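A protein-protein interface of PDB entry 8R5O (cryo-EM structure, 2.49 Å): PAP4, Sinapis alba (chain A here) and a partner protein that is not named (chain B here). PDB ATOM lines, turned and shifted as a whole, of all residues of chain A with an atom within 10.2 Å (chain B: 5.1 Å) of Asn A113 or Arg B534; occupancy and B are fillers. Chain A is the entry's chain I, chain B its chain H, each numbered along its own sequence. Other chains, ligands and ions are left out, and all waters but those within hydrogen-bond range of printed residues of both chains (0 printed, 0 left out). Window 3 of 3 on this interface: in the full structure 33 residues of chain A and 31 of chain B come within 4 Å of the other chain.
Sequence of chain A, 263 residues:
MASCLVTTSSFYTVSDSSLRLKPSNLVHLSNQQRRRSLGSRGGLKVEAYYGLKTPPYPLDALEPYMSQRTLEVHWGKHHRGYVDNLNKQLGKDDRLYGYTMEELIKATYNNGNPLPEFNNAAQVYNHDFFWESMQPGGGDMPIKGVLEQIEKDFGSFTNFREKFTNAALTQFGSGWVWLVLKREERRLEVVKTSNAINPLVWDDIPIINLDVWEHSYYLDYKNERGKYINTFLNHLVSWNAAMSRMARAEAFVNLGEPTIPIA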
ATOM      1  N   ILE A 105      -7.604   4.238 -13.398  1.00  0.00           N
ATOM      2  CA  ILE A 105      -6.698   3.093 -13.333  1.00  0.00           C
ATOM      3  C   ILE A 105      -5.670   3.284 -12.228  1.00  0.00           C
ATOM      4  O   ILE A 105      -5.391   2.363 -11.451  1.00  0.00           O
ATOM      5  CB  ILE A 105      -6.028   2.871 -14.700  1.00  0.00           C
ATOM      6  CG1 ILE A 105      -7.071   2.459 -15.735  1.00  0.00           C
ATOM      7  CG2 ILE A 105      -4.929   1.825 -14.598  1.00  0.00           C
ATOM      8  CD1 ILE A 105      -6.509   2.307 -17.114  1.00  0.00           C
ATOM      9  N   LYS A 106      -5.087   4.481 -12.140  1.00  0.00           N
ATOM     10  CA  LYS A 106      -4.095   4.748 -11.104  1.00  0.00           C
ATOM     11  C   LYS A 106      -4.722   4.741  -9.717  1.00  0.00           C
ATOM     12  O   LYS A 106      -4.116   4.249  -8.758  1.00  0.00           O
ATOM     13  CB  LYS A 106      -3.401   6.081 -11.383  1.00  0.00           C
ATOM     14  CG  LYS A 106      -2.581   6.073 -12.662  1.00  0.00           C
ATOM     15  CD  LYS A 106      -2.486   7.454 -13.291  1.00  0.00           C
ATOM     16  CE  LYS A 106      -1.827   7.380 -14.660  1.00  0.00           C
ATOM     17  NZ  LYS A 106      -1.884   8.675 -15.388  1.00  0.00           N
ATOM     18  N   ALA A 107      -5.934   5.284  -9.586  1.00  0.00           N
ATOM     19  CA  ALA A 107      -6.591   5.323  -8.283  1.00  0.00           C
ATOM     20  C   ALA A 107      -6.996   3.927  -7.826  1.00  0.00           C
ATOM     21  O   ALA A 107      -6.782   3.559  -6.664  1.00  0.00           O
ATOM     22  CB  ALA A 107      -7.809   6.246  -8.336  1.00  0.00           C
ATOM     23  N   THR A 108      -7.583   3.133  -8.723  1.00  0.00           N
ATOM     24  CA  THR A 108      -8.016   1.790  -8.351  1.00  0.00           C
ATOM     25  C   THR A 108      -6.849   0.832  -8.165  1.00  0.00           C
ATOM     26  O   THR A 108      -7.006  -0.189  -7.489  1.00  0.00           O
ATOM     27  CB  THR A 108      -8.983   1.229  -9.394  1.00  0.00           C
ATOM     28  OG1 THR A 108      -8.399   1.329 -10.697  1.00  0.00           O
ATOM     29  CG2 THR A 108     -10.296   1.992  -9.369  1.00  0.00           C
ATOM     30  N   TYR A 109      -5.686   1.131  -8.748  1.00  0.00           N
ATOM     31  CA  TYR A 109      -4.507   0.312  -8.485  1.00  0.00           C
ATOM     32  C   TYR A 109      -4.093   0.408  -7.025  1.00  0.00           C
ATOM     33  O   TYR A 109      -3.586  -0.566  -6.458  1.00  0.00           O
ATOM     34  CB  TYR A 109      -3.360   0.728  -9.404  1.00  0.00           C
ATOM     35  CG  TYR A 109      -2.093  -0.069  -9.201  1.00  0.00           C
ATOM     36  CD1 TYR A 109      -2.024  -1.405  -9.574  1.00  0.00           C
ATOM     37  CD2 TYR A 109      -0.964   0.515  -8.646  1.00  0.00           C
ATOM     38  CE1 TYR A 109      -0.870  -2.135  -9.393  1.00  0.00           C
ATOM     39  CE2 TYR A 109       0.195  -0.209  -8.463  1.00  0.00           C
ATOM     40  CZ  TYR A 109       0.237  -1.534  -8.837  1.00  0.00           C
ATOM     41  OH  TYR A 109       1.388  -2.261  -8.658  1.00  0.00           O
ATOM     42  N   ASN A 110      -4.302   1.573  -6.406  1.00  0.00           N
ATOM     43  CA  ASN A 110      -4.158   1.753  -4.960  1.00  0.00           C
ATOM     44  C   ASN A 110      -2.754   1.390  -4.479  1.00  0.00           C
ATOM     45  O   ASN A 110      -2.579   0.781  -3.421  1.00  0.00           O
ATOM     46  CB  ASN A 110      -5.222   0.952  -4.205  1.00  0.00           C
ATOM     47  CG  ASN A 110      -5.407   1.424  -2.779  1.00  0.00           C
ATOM     48  OD1 ASN A 110      -5.216   2.598  -2.471  1.00  0.00           O
ATOM     49  ND2 ASN A 110      -5.779   0.505  -1.897  1.00  0.00           N
ATOM     50  N   ASN A 111      -1.747   1.765  -5.269  1.00  0.00           N
ATOM     51  CA  ASN A 111      -0.340   1.621  -4.892  1.00  0.00           C
ATOM     52  C   ASN A 111       0.017   0.174  -4.549  1.00  0.00           C
ATOM     53  O   ASN A 111       0.767  -0.093  -3.610  1.00  0.00           O
ATOM     54  CB  ASN A 111       0.016   2.558  -3.735  1.00  0.00           C
ATOM     55  CG  ASN A 111       1.507   2.798  -3.615  1.00  0.00           C
ATOM     56  OD1 ASN A 111       2.228   2.814  -4.612  1.00  0.00           O
ATOM     57  ND2 ASN A 111       1.981   2.984  -2.388  1.00  0.00           N
ATOM     58  N   GLY A 112      -0.531  -0.771  -5.308  1.00  0.00           N
ATOM     59  CA  GLY A 112      -0.195  -2.170  -5.147  1.00  0.00           C
ATOM     60  C   GLY A 112      -1.189  -3.007  -4.372  1.00  0.00           C
ATOM     61  O   GLY A 112      -0.926  -4.194  -4.152  1.00  0.00           O
ATOM     62  N   ASN A 113      -2.316  -2.438  -3.955  1.00  0.00           N
ATOM     63  CA  ASN A 113      -3.395  -3.185  -3.307  1.00  0.00           C
ATOM     64  C   ASN A 113      -4.690  -2.871  -4.046  1.00  0.00           C
ATOM     65  O   ASN A 113      -5.542  -2.126  -3.549  1.00  0.00           O
ATOM     66  CB  ASN A 113      -3.496  -2.836  -1.823  1.00  0.00           C
ATOM     67  CG  ASN A 113      -4.433  -3.756  -1.069  1.00  0.00           C
ATOM     68  OD1 ASN A 113      -4.734  -4.860  -1.520  1.00  0.00           O
ATOM     69  ND2 ASN A 113      -4.898  -3.305   0.088  1.00  0.00           N
ATOM     70  N   PRO A 114      -4.869  -3.436  -5.242  1.00  0.00           N
ATOM     71  CA  PRO A 114      -5.917  -2.949  -6.148  1.00  0.00           C
ATOM     72  C   PRO A 114      -7.320  -3.095  -5.578  1.00  0.00           C
ATOM     73  O   PRO A 114      -7.645  -4.075  -4.905  1.00  0.00           O
ATOM     74  CB  PRO A 114      -5.732  -3.816  -7.398  1.00  0.00           C
ATOM     75  CG  PRO A 114      -4.323  -4.296  -7.323  1.00  0.00           C
ATOM     76  CD  PRO A 114      -4.048  -4.486  -5.866  1.00  0.00           C
ATOM     77  N   LEU A 115      -8.153  -2.100  -5.867  1.00  0.00           N
ATOM     78  CA  LEU A 115      -9.567  -2.113  -5.538  1.00  0.00           C
ATOM     79  C   LEU A 115     -10.319  -3.036  -6.493  1.00  0.00           C
ATOM     80  O   LEU A 115      -9.799  -3.401  -7.550  1.00  0.00           O
ATOM     81  CB  LEU A 115     -10.123  -0.693  -5.604  1.00  0.00           C
ATOM     82  CG  LEU A 115      -9.454   0.332  -4.686  1.00  0.00           C
ATOM     83  CD1 LEU A 115     -10.152   1.678  -4.777  1.00  0.00           C
ATOM     84  CD2 LEU A 115      -9.426  -0.165  -3.249  1.00  0.00           C
ATOM     85  N   PRO A 116     -11.543  -3.444  -6.141  1.00  0.00           N
ATOM     86  CA  PRO A 116     -12.281  -4.378  -7.013  1.00  0.00           C
ATOM     87  C   PRO A 116     -12.514  -3.865  -8.424  1.00  0.00           C
ATOM     88  O   PRO A 116     -12.679  -4.680  -9.340  1.00  0.00           O
ATOM     89  CB  PRO A 116     -13.608  -4.574  -6.268  1.00  0.00           C
ATOM     90  CG  PRO A 116     -13.279  -4.311  -4.848  1.00  0.00           C
ATOM     91  CD  PRO A 116     -12.245  -3.225  -4.863  1.00  0.00           C
ATOM     92  N   GLU A 117     -12.538  -2.551  -8.636  1.00  0.00           N
ATOM     93  CA  GLU A 117     -12.788  -2.007  -9.964  1.00  0.00           C
ATOM     94  C   GLU A 117     -11.552  -1.995 -10.854  1.00  0.00           C
ATOM     95  O   GLU A 117     -11.681  -1.725 -12.052  1.00  0.00           O
ATOM     96  CB  GLU A 117     -13.343  -0.583  -9.855  1.00  0.00           C
ATOM     97  CG  GLU A 117     -14.710  -0.484  -9.195  1.00  0.00           C
ATOM     98  CD  GLU A 117     -14.646  -0.561  -7.681  1.00  0.00           C
ATOM     99  OE1 GLU A 117     -13.533  -0.465  -7.124  1.00  0.00           O
ATOM    100  OE2 GLU A 117     -15.711  -0.719  -7.047  1.00  0.00           O
ATOM    101  N   PHE A 118     -10.366  -2.279 -10.307  1.00  0.00           N
ATOM    102  CA  PHE A 118      -9.136  -2.121 -11.076  1.00  0.00           C
ATOM    103  C   PHE A 118      -9.084  -3.065 -12.272  1.00  0.00           C
ATOM    104  O   PHE A 118      -8.680  -2.659 -13.366  1.00  0.00           O
ATOM    105  CB  PHE A 118      -7.913  -2.338 -10.186  1.00  0.00           C
ATOM    106  CG  PHE A 118      -6.618  -2.375 -10.948  1.00  0.00           C
ATOM    107  CD1 PHE A 118      -6.043  -1.206 -11.417  1.00  0.00           C
ATOM    108  CD2 PHE A 118      -5.983  -3.578 -11.209  1.00  0.00           C
ATOM    109  CE1 PHE A 118      -4.861  -1.236 -12.125  1.00  0.00           C
ATOM    110  CE2 PHE A 118      -4.799  -3.613 -11.917  1.00  0.00           C
ATOM    111  CZ  PHE A 118      -4.237  -2.440 -12.375  1.00  0.00           C
ATOM    112  N   ASN A 119      -9.474  -4.328 -12.083  1.00  0.00           N
ATOM    113  CA  ASN A 119      -9.325  -5.308 -13.156  1.00  0.00           C
ATOM    114  C   ASN A 119     -10.158  -4.934 -14.375  1.00  0.00           C
ATOM    115  O   ASN A 119      -9.686  -5.034 -15.511  1.00  0.00           O
ATOM    116  CB  ASN A 119      -9.699  -6.704 -12.661  1.00  0.00           C
ATOM    117  CG  ASN A 119      -8.608  -7.337 -11.824  1.00  0.00           C
ATOM    118  OD1 ASN A 119      -7.457  -6.908 -11.858  1.00  0.00           O
ATOM    119  ND2 ASN A 119      -8.965  -8.370 -11.072  1.00  0.00           N
ATOM    120  N   SER A 194       1.625  -8.703 -15.695  1.00  0.00           N
ATOM    121  CA  SER A 194       0.761  -9.859 -15.506  1.00  0.00           C
ATOM    122  C   SER A 194      -0.684  -9.418 -15.318  1.00  0.00           C
ATOM    123  O   SER A 194      -0.953  -8.386 -14.695  1.00  0.00           O
ATOM    124  CB  SER A 194       1.211 -10.689 -14.301  1.00  0.00           C
ATOM    125  OG  SER A 194       1.100  -9.947 -13.100  1.00  0.00           O
ATOM    126  N   ASN A 195      -1.606 -10.210 -15.868  1.00  0.00           N
ATOM    127  CA  ASN A 195      -3.054 -10.005 -15.743  1.00  0.00           C
ATOM    128  C   ASN A 195      -3.415  -8.661 -16.367  1.00  0.00           C
ATOM    129  O   ASN A 195      -3.170  -8.481 -17.572  1.00  0.00           O
ATOM    130  CB  ASN A 195      -3.457 -10.190 -14.278  1.00  0.00           C
ATOM    131  CG  ASN A 195      -3.382 -11.636 -13.833  1.00  0.00           C
ATOM    132  OD1 ASN A 195      -2.952 -12.508 -14.585  1.00  0.00           O
ATOM    133  ND2 ASN A 195      -3.796 -11.897 -12.600  1.00  0.00           N
ATOM    134  N   ILE A 197      -2.386  -5.500 -15.355  1.00  0.00           N
ATOM    135  CA  ILE A 197      -1.509  -4.389 -15.006  1.00  0.00           C
ATOM    136  C   ILE A 197      -0.975  -3.729 -16.271  1.00  0.00           C
ATOM    137  O   ILE A 197      -0.594  -4.403 -17.237  1.00  0.00           O
ATOM    138  CB  ILE A 197      -0.372  -4.882 -14.096  1.00  0.00           C
ATOM    139  CG1 ILE A 197      -0.949  -5.395 -12.777  1.00  0.00           C
ATOM    140  CG2 ILE A 197       0.638  -3.777 -13.836  1.00  0.00           C
ATOM    141  CD1 ILE A 197       0.094  -5.878 -11.807  1.00  0.00           C
ATOM    142  N   VAL A 201       0.096   2.686 -14.110  1.00  0.00           N
ATOM    143  CA  VAL A 201       0.164   2.676 -12.653  1.00  0.00           C
ATOM    144  C   VAL A 201       1.511   3.145 -12.125  1.00  0.00           C
ATOM    145  O   VAL A 201       1.620   3.467 -10.938  1.00  0.00           O
ATOM    146  CB  VAL A 201      -0.160   1.271 -12.106  1.00  0.00           C
ATOM    147  CG1 VAL A 201      -1.491   0.785 -12.655  1.00  0.00           C
ATOM    148  CG2 VAL A 201       0.951   0.294 -12.446  1.00  0.00           C
ATOM    149  N   TRP A 202       2.539   3.195 -12.976  1.00  0.00           N
ATOM    150  CA  TRP A 202       3.838   3.741 -12.602  1.00  0.00           C
ATOM    151  C   TRP A 202       4.169   5.005 -13.386  1.00  0.00           C
ATOM    152  O   TRP A 202       5.347   5.339 -13.546  1.00  0.00           O
ATOM    153  CB  TRP A 202       4.939   2.695 -12.792  1.00  0.00           C
ATOM    154  CG  TRP A 202       4.630   1.393 -12.137  1.00  0.00           C
ATOM    155  CD1 TRP A 202       4.431   1.173 -10.806  1.00  0.00           C
ATOM    156  CD2 TRP A 202       4.482   0.125 -12.782  1.00  0.00           C
ATOM    157  NE1 TRP A 202       4.167  -0.156 -10.580  1.00  0.00           N
ATOM    158  CE2 TRP A 202       4.192  -0.821 -11.778  1.00  0.00           C
ATOM    159  CE3 TRP A 202       4.564  -0.303 -14.109  1.00  0.00           C
ATOM    160  CZ2 TRP A 202       3.985  -2.168 -12.062  1.00  0.00           C
ATOM    161  CZ3 TRP A 202       4.358  -1.641 -14.388  1.00  0.00           C
ATOM    162  CH2 TRP A 202       4.072  -2.557 -13.369  1.00  0.00           C
ATOM    163  N   ASP B 530      -1.260 -14.724   0.739  1.00  0.00           N
ATOM    164  CA  ASP B 530      -1.137 -13.435   0.065  1.00  0.00           C
ATOM    165  C   ASP B 530       0.252 -13.255  -0.533  1.00  0.00           C
ATOM    166  O   ASP B 530       0.401 -12.654  -1.603  1.00  0.00           O
ATOM    167  CB  ASP B 530      -1.456 -12.302   1.041  1.00  0.00           C
ATOM    168  CG  ASP B 530      -1.562 -10.956   0.356  1.00  0.00           C
ATOM    169  OD1 ASP B 530      -2.538 -10.743  -0.391  1.00  0.00           O
ATOM    170  OD2 ASP B 530      -0.668 -10.109   0.563  1.00  0.00           O
ATOM    171  N   ILE B 531       1.282 -13.763   0.145  1.00  0.00           N
ATOM    172  CA  ILE B 531       2.643 -13.659  -0.374  1.00  0.00           C
ATOM    173  C   ILE B 531       2.781 -14.445  -1.673  1.00  0.00           C
ATOM    174  O   ILE B 531       3.354 -13.959  -2.654  1.00  0.00           O
ATOM    175  CB  ILE B 531       3.658 -14.128   0.685  1.00  0.00           C
ATOM    176  CG1 ILE B 531       3.769 -13.095   1.805  1.00  0.00           C
ATOM    177  CG2 ILE B 531       5.018 -14.383   0.059  1.00  0.00           C
ATOM    178  CD1 ILE B 531       4.686 -13.512   2.926  1.00  0.00           C
ATOM    179  N   SER B 532       2.245 -15.667  -1.703  1.00  0.00           N
ATOM    180  CA  SER B 532       2.378 -16.503  -2.894  1.00  0.00           C
ATOM    181  C   SER B 532       1.666 -15.886  -4.092  1.00  0.00           C
ATOM    182  O   SER B 532       2.178 -15.939  -5.216  1.00  0.00           O
ATOM    183  CB  SER B 532       1.848 -17.910  -2.615  1.00  0.00           C
ATOM    184  OG  SER B 532       0.471 -17.895  -2.293  1.00  0.00           O
ATOM    185  N   SER B 533       0.484 -15.305  -3.876  1.00  0.00           N
ATOM    186  CA  SER B 533      -0.237 -14.661  -4.972  1.00  0.00           C
ATOM    187  C   SER B 533       0.517 -13.443  -5.492  1.00  0.00           C
ATOM    188  O   SER B 533       0.634 -13.246  -6.706  1.00  0.00           O
ATOM    189  CB  SER B 533      -1.643 -14.267  -4.517  1.00  0.00           C
ATOM    190  OG  SER B 533      -2.392 -15.403  -4.129  1.00  0.00           O
ATOM    191  N   ARG B 534       1.033 -12.610  -4.585  1.00  0.00           N
ATOM    192  CA  ARG B 534       1.713 -11.389  -5.004  1.00  0.00           C
ATOM    193  C   ARG B 534       3.042 -11.691  -5.686  1.00  0.00           C
ATOM    194  O   ARG B 534       3.421 -11.007  -6.642  1.00  0.00           O
ATOM    195  CB  ARG B 534       1.918 -10.467  -3.804  1.00  0.00           C
ATOM    196  CG  ARG B 534       0.629  -9.860  -3.288  1.00  0.00           C
ATOM    197  CD  ARG B 534       0.868  -8.944  -2.107  1.00  0.00           C
ATOM    198  NE  ARG B 534      -0.356  -8.251  -1.724  1.00  0.00           N
ATOM    199  CZ  ARG B 534      -0.734  -7.077  -2.209  1.00  0.00           C
ATOM    200  NH1 ARG B 534       0.010  -6.417  -3.080  1.00  0.00           N
ATOM    201  NH2 ARG B 534      -1.887  -6.551  -1.808  1.00  0.00           N
ATOM    202  N   GLN B 535       3.767 -12.703  -5.206  1.00  0.00           N
ATOM    203  CA  GLN B 535       5.024 -13.071  -5.850  1.00  0.00           C
ATOM    204  C   GLN B 535       4.794 -13.643  -7.243  1.00  0.00           C
ATOM    205  O   GLN B 535       5.635 -13.464  -8.130  1.00  0.00           O
ATOM    206  CB  GLN B 535       5.789 -14.073  -4.985  1.00  0.00           C
ATOM    207  CG  GLN B 535       6.302 -13.512  -3.665  1.00  0.00           C
ATOM    208  CD  GLN B 535       7.598 -12.735  -3.806  1.00  0.00           C
ATOM    209  OE1 GLN B 535       7.776 -11.959  -4.743  1.00  0.00           O
ATOM    210  NE2 GLN B 535       8.514 -12.945  -2.870  1.00  0.00           N
ATOM    211  N   ALA B 536       3.671 -14.329  -7.453  1.00  0.00           N
ATOM    212  CA  ALA B 536       3.371 -14.887  -8.766  1.00  0.00           C
ATOM    213  C   ALA B 536       2.927 -13.811  -9.749  1.00  0.00           C
ATOM    214  O   ALA B 536       3.226 -13.900 -10.946  1.00  0.00           O
ATOM    215  CB  ALA B 536       2.300 -15.969  -8.644  1.00  0.00           C
ATOM    216  N   LEU B 537       2.216 -12.795  -9.271  1.00  0.00           N
ATOM    217  CA  LEU B 537       1.658 -11.756 -10.125  1.00  0.00           C
ATOM    218  C   LEU B 537       2.497 -10.486 -10.150  1.00  0.00           C
ATOM    219  O   LEU B 537       2.080  -9.499 -10.764  1.00  0.00           O
ATOM    220  CB  LEU B 537       0.230 -11.430  -9.682  1.00  0.00           C
ATOM    221  CG  LEU B 537      -0.734 -12.616  -9.706  1.00  0.00           C
ATOM    222  CD1 LEU B 537      -2.057 -12.249  -9.065  1.00  0.00           C
ATOM    223  CD2 LEU B 537      -0.944 -13.103 -11.131  1.00  0.00           C
ATOM    224  N   GLY B 538       3.658 -10.484  -9.505  1.00  0.00           N
ATOM    225  CA  GLY B 538       4.514  -9.308  -9.507  1.00  0.00           C
ATOM    226  C   GLY B 538       3.925  -8.110  -8.798  1.00  0.00           C
ATOM    227  O   GLY B 538       4.093  -6.975  -9.259  1.00  0.00           O
ATOM    228  N   LEU B 539       3.238  -8.334  -7.685  1.00  0.00           N
ATOM    229  CA  LEU B 539       2.680  -7.273  -6.866  1.00  0.00           C
ATOM    230  C   LEU B 539       3.565  -7.019  -5.650  1.00  0.00           C
ATOM    231  O   LEU B 539       4.190  -7.946  -5.127  1.00  0.00           O
ATOM    232  CB  LEU B 539       1.265  -7.633  -6.406  1.00  0.00           C
ATOM    233  CG  LEU B 539       0.189  -7.629  -7.494  1.00  0.00           C
ATOM    234  CD1 LEU B 539      -1.072  -8.313  -7.002  1.00  0.00           C
ATOM    235  CD2 LEU B 539      -0.115  -6.208  -7.933  1.00  0.00           C
ATOM    236  N   PRO B 540       3.649  -5.774  -5.185  1.00  0.00           N
ATOM    237  CA  PRO B 540       4.556  -5.466  -4.073  1.00  0.00           C
ATOM    238  C   PRO B 540       4.151  -6.178  -2.790  1.00  0.00           C
ATOM    239  O   PRO B 540       2.967  -6.338  -2.491  1.00  0.00           O
ATOM    240  CB  PRO B 540       4.438  -3.945  -3.933  1.00  0.00           C
ATOM    241  CG  PRO B 540       3.103  -3.620  -4.505  1.00  0.00           C
ATOM    242  CD  PRO B 540       2.903  -4.585  -5.633  1.00  0.00           C
ATOM    243  N   LEU B 541       5.158  -6.608  -2.031  1.00  0.00           N
ATOM    244  CA  LEU B 541       4.930  -7.194  -0.716  1.00  0.00           C
ATOM    245  C   LEU B 541       4.871  -6.144   0.382  1.00  0.00           C
ATOM    246  O   LEU B 541       4.112  -6.304   1.344  1.00  0.00           O
ATOM    247  CB  LEU B 541       6.026  -8.213  -0.394  1.00  0.00           C
ATOM    248  CG  LEU B 541       6.079  -9.445  -1.297  1.00  0.00           C
ATOM    249  CD1 LEU B 541       7.187 -10.385  -0.852  1.00  0.00           C
ATOM    250  CD2 LEU B 541       4.736 -10.155  -1.305  1.00  0.00           C
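NH1 of Arg B534 lies within hydrogen-bond range of O of Gly A112 (2.6 Å). The guanidinium group (NH2) of Arg B534 lies within hydrogen-bond range of the side-chain amide oxygen (OD1) of Asn A113. The side-chain hydroxyl of Ser A194 sits at hydrogen-bond distance from the backbone carbonyl oxygen of Leu B537 (2.6 Å).
The side-chain carboxylate (OD2) of Asp B530 lies within salt-bridge range of the guanidinium group (NE) of Arg B534. O of Arg B534 lies within hydrogen-bond range of N of Leu B539. NH1 of Arg B534 sits at hydrogen-bond distance from O of Pro B540 (3.0 Å). The side-chain amide nitrogen (ND2) of Asn A110 is in hydrogen-bond range of the backbone carbonyl oxygen (O) of Asn A113, at 3.1 Å.
Among the printed residues, pairs that only touch across the chains: Asn A195 with Leu B537 (3.4 Å), Gly A112 with Pro B540 (3.7 Å) and Ile A197 with Leu B539 (3.9 Å).
Of chain A, only Gly A112 and Asn A113 come within 4 Å of Arg B534. Ser B532 touches none of the printed residues of chain A. No residue of chain A comes within 4 Å of Ser B533. No residue of chain A comes within 4 Å of Ala B536. No residue of chain A comes within 4 Å of Gly B538. Leu B539 touches just one residue of chain A: Ile A197 (3.9 Å). Of chain A, only Gly A112 comes within 4 Å of Pro B540. Printed residues of chain A within 4 Å of Leu B537: Ser A194 and Asn A195. Printed residues of chain B within 4 Å of Gly A112: Arg B534 (2.6 Å) and Pro B540 (3.7 Å). Printed residues of chain B within 4 Å of Ile A197: Leu B539 (3.9 Å). The nearest printed residue of chain B that does not touch Asn A113 is Pro B540 (5.6 Å). The nearest printed residue of chain B that does not touch Ile A197 is Leu B537 (4.3 Å).
Of the 20 printed residues of chain A, 5 touch a printed residue of chain B. Along chain A the printed residues that touch a printed residue of chain B span positions 112 to 197. Of the 12 printed residues of chain B, 4 touch a printed residue of chain A. Hydrophobic or aromatic side chains of chain B within 4 Å of the printed part of chain A: Leu B537, Leu B539 and Pro B540. Among the printed residues, 6 pairs touch across the chains. Among the printed residues, no Asp or Glu carboxylate lies within 4 Å of a Lys or Arg side-chain nitrogen of the other chain.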
